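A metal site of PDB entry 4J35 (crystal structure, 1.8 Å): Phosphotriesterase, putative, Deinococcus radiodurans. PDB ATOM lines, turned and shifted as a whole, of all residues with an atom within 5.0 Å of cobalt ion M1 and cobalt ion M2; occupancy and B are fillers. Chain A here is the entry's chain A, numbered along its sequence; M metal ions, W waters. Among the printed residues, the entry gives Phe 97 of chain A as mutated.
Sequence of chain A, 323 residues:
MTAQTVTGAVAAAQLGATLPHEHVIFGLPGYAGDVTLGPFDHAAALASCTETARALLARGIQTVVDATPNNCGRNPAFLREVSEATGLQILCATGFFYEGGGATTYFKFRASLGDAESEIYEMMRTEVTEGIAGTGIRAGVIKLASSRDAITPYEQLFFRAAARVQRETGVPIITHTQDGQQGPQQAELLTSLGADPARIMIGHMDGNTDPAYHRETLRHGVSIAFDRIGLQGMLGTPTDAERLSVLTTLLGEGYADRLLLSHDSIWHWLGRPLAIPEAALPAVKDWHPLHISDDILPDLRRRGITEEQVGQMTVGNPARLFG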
ATOM      1  N   HIS A  21      -9.702  -4.832   9.680  1.00  0.00           N
ATOM      2  CA  HIS A  21      -9.855  -6.283   9.672  1.00  0.00           C
ATOM      3  C   HIS A  21      -9.933  -6.759   8.219  1.00  0.00           C
ATOM      4  O   HIS A  21     -10.998  -6.707   7.630  1.00  0.00           O
ATOM      5  CB  HIS A  21     -11.130  -6.757  10.368  1.00  0.00           C
ATOM      6  CG  HIS A  21     -11.186  -8.239  10.571  1.00  0.00           C
ATOM      7  ND1 HIS A  21     -11.418  -8.826  11.809  1.00  0.00           N
ATOM      8  CD2 HIS A  21     -11.078  -9.278   9.706  1.00  0.00           C
ATOM      9  CE1 HIS A  21     -11.424 -10.129  11.677  1.00  0.00           C
ATOM     10  NE2 HIS A  21     -11.278 -10.424  10.396  1.00  0.00           N
ATOM     11  N   HIS A  23      -7.612  -9.712   5.297  1.00  0.00           N
ATOM     12  CA  HIS A  23      -6.735 -10.865   5.184  1.00  0.00           C
ATOM     13  C   HIS A  23      -5.948 -10.742   3.847  1.00  0.00           C
ATOM     14  O   HIS A  23      -6.502 -10.992   2.803  1.00  0.00           O
ATOM     15  CB  HIS A  23      -7.574 -12.173   5.263  1.00  0.00           C
ATOM     16  CG  HIS A  23      -8.249 -12.348   6.611  1.00  0.00           C
ATOM     17  ND1 HIS A  23      -7.524 -12.700   7.733  1.00  0.00           N
ATOM     18  CD2 HIS A  23      -9.525 -12.173   7.037  1.00  0.00           C
ATOM     19  CE1 HIS A  23      -8.325 -12.765   8.771  1.00  0.00           C
ATOM     20  NE2 HIS A  23      -9.544 -12.399   8.399  1.00  0.00           N
ATOM     21  N   ALA A  67      -5.819  -9.604  10.090  1.00  0.00           N
ATOM     22  CA  ALA A  67      -6.376 -10.307  11.278  1.00  0.00           C
ATOM     23  C   ALA A  67      -6.151 -11.810  11.222  1.00  0.00           C
ATOM     24  O   ALA A  67      -6.736 -12.573  11.974  1.00  0.00           O
ATOM     25  CB  ALA A  67      -7.847 -10.014  11.358  1.00  0.00           C
ATOM     26  N   PHE A  97      -7.663 -19.518  15.819  1.00  0.00           N
ATOM     27  CA  PHE A  97      -9.063 -19.364  15.388  1.00  0.00           C
ATOM     28  C   PHE A  97     -10.050 -20.150  16.271  1.00  0.00           C
ATOM     29  O   PHE A  97      -9.651 -21.038  17.015  1.00  0.00           O
ATOM     30  CB  PHE A  97      -9.139 -19.829  13.926  1.00  0.00           C
ATOM     31  CG  PHE A  97     -10.272 -19.268  13.148  1.00  0.00           C
ATOM     32  CD1 PHE A  97     -10.559 -17.902  13.141  1.00  0.00           C
ATOM     33  CD2 PHE A  97     -11.001 -20.107  12.307  1.00  0.00           C
ATOM     34  CE1 PHE A  97     -11.592 -17.385  12.354  1.00  0.00           C
ATOM     35  CE2 PHE A  97     -12.039 -19.582  11.505  1.00  0.00           C
ATOM     36  CZ  PHE A  97     -12.325 -18.224  11.535  1.00  0.00           C
ATOM     37  N   KCX A 143      -5.548 -11.433  18.241  1.00  0.00           N
ATOM     38  CA  KCX A 143      -6.747 -11.943  17.617  1.00  0.00           C
ATOM     39  CB  KCX A 143      -6.513 -12.391  16.167  1.00  0.00           C
ATOM     40  CG  KCX A 143      -7.698 -13.077  15.517  1.00  0.00           C
ATOM     41  CD  KCX A 143      -8.802 -12.108  15.086  1.00  0.00           C
ATOM     42  CE  KCX A 143      -9.970 -12.859  14.475  1.00  0.00           C
ATOM     43  NZ  KCX A 143      -9.738 -13.052  12.949  1.00  0.00           N
ATOM     44  C   KCX A 143      -7.357 -13.039  18.466  1.00  0.00           C
ATOM     45  O   KCX A 143      -6.732 -14.081  18.757  1.00  0.00           O
ATOM     46  CX  KCX A 143     -10.616 -13.233  11.992  1.00  0.00           C
ATOM     47  OQ1 KCX A 143     -10.038 -13.352  10.869  1.00  0.00           O
ATOM     48  OQ2 KCX A 143     -11.878 -13.360  12.053  1.00  0.00           O
ATOM     49  N   HIS A 176     -13.168 -12.103  16.514  1.00  0.00           N
ATOM     50  CA  HIS A 176     -14.112 -12.735  15.623  1.00  0.00           C
ATOM     51  C   HIS A 176     -15.321 -13.181  16.443  1.00  0.00           C
ATOM     52  O   HIS A 176     -15.143 -13.810  17.484  1.00  0.00           O
ATOM     53  CB  HIS A 176     -13.432 -13.960  14.978  1.00  0.00           C
ATOM     54  CG  HIS A 176     -14.360 -14.929  14.286  1.00  0.00           C
ATOM     55  ND1 HIS A 176     -14.410 -15.098  12.932  1.00  0.00           N
ATOM     56  CD2 HIS A 176     -15.204 -15.865  14.806  1.00  0.00           C
ATOM     57  CE1 HIS A 176     -15.286 -16.047  12.626  1.00  0.00           C
ATOM     58  NE2 HIS A 176     -15.785 -16.520  13.738  1.00  0.00           N
ATOM     59  N   HIS A 204     -16.975  -8.545  13.712  1.00  0.00           N
ATOM     60  CA  HIS A 204     -18.099  -9.133  13.006  1.00  0.00           C
ATOM     61  C   HIS A 204     -19.459  -8.782  13.618  1.00  0.00           C
ATOM     62  O   HIS A 204     -20.411  -9.580  13.550  1.00  0.00           O
ATOM     63  CB  HIS A 204     -17.913 -10.664  12.858  1.00  0.00           C
ATOM     64  CG  HIS A 204     -16.589 -11.095  12.296  1.00  0.00           C
ATOM     65  ND1 HIS A 204     -15.827 -10.297  11.464  1.00  0.00           N
ATOM     66  CD2 HIS A 204     -15.899 -12.254  12.432  1.00  0.00           C
ATOM     67  CE1 HIS A 204     -14.726 -10.955  11.108  1.00  0.00           C
ATOM     68  NE2 HIS A 204     -14.747 -12.141  11.698  1.00  0.00           N
ATOM     69  N   ASP A 264     -13.212  -7.772   5.864  1.00  0.00           N
ATOM     70  CA  ASP A 264     -12.825  -9.166   6.111  1.00  0.00           C
ATOM     71  C   ASP A 264     -12.524  -9.870   4.773  1.00  0.00           C
ATOM     72  O   ASP A 264     -12.768 -11.055   4.612  1.00  0.00           O
ATOM     73  CB  ASP A 264     -13.936  -9.893   6.840  1.00  0.00           C
ATOM     74  CG  ASP A 264     -13.461 -11.182   7.509  1.00  0.00           C
ATOM     75  OD1 ASP A 264     -12.247 -11.418   7.673  1.00  0.00           O
ATOM     76  OD2 ASP A 264     -14.345 -11.986   7.834  1.00  0.00           O
HETATM   77 CO    CO M   1     -11.226 -12.332   9.410  1.00  0.00          CO
HETATM   78 CO    CO M   2     -13.531 -13.722  11.534  1.00  0.00          CO
HETATM   79  O   HOH W   1     -15.835 -14.663   9.832  1.00  0.00           O
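The backbone carbonyl oxygen (O) of Ala 67 is in hydrogen-bond range of NZ of KCX 143.
Within 4 Å of cobalt ion M1: His 21, His 23, KCX 143 and Asp 264.
The nearest printed residue that does not touch cobalt ion M1 is His 204 (4.1 Å).
Within 4 Å of cobalt ion M2: KCX 143, His 176 and His 204.
Cobalt ion M1 is bound by NE2 of His 23 (2.0 Å), OQ1 of KCX 143 (2.1 Å), NE2 of His 21 (2.1 Å) and OD1 of Asp 264 (2.2 Å).
Cobalt ion M1 has four donor atoms within binding distance.
Cobalt ion M2 is bound by OQ2 of KCX 143 (1.8 Å), NE2 of His 204 (2.0 Å) and ND1 of His 176 (2.1 Å).
Cobalt ion M2 has three donor atoms within binding distance.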
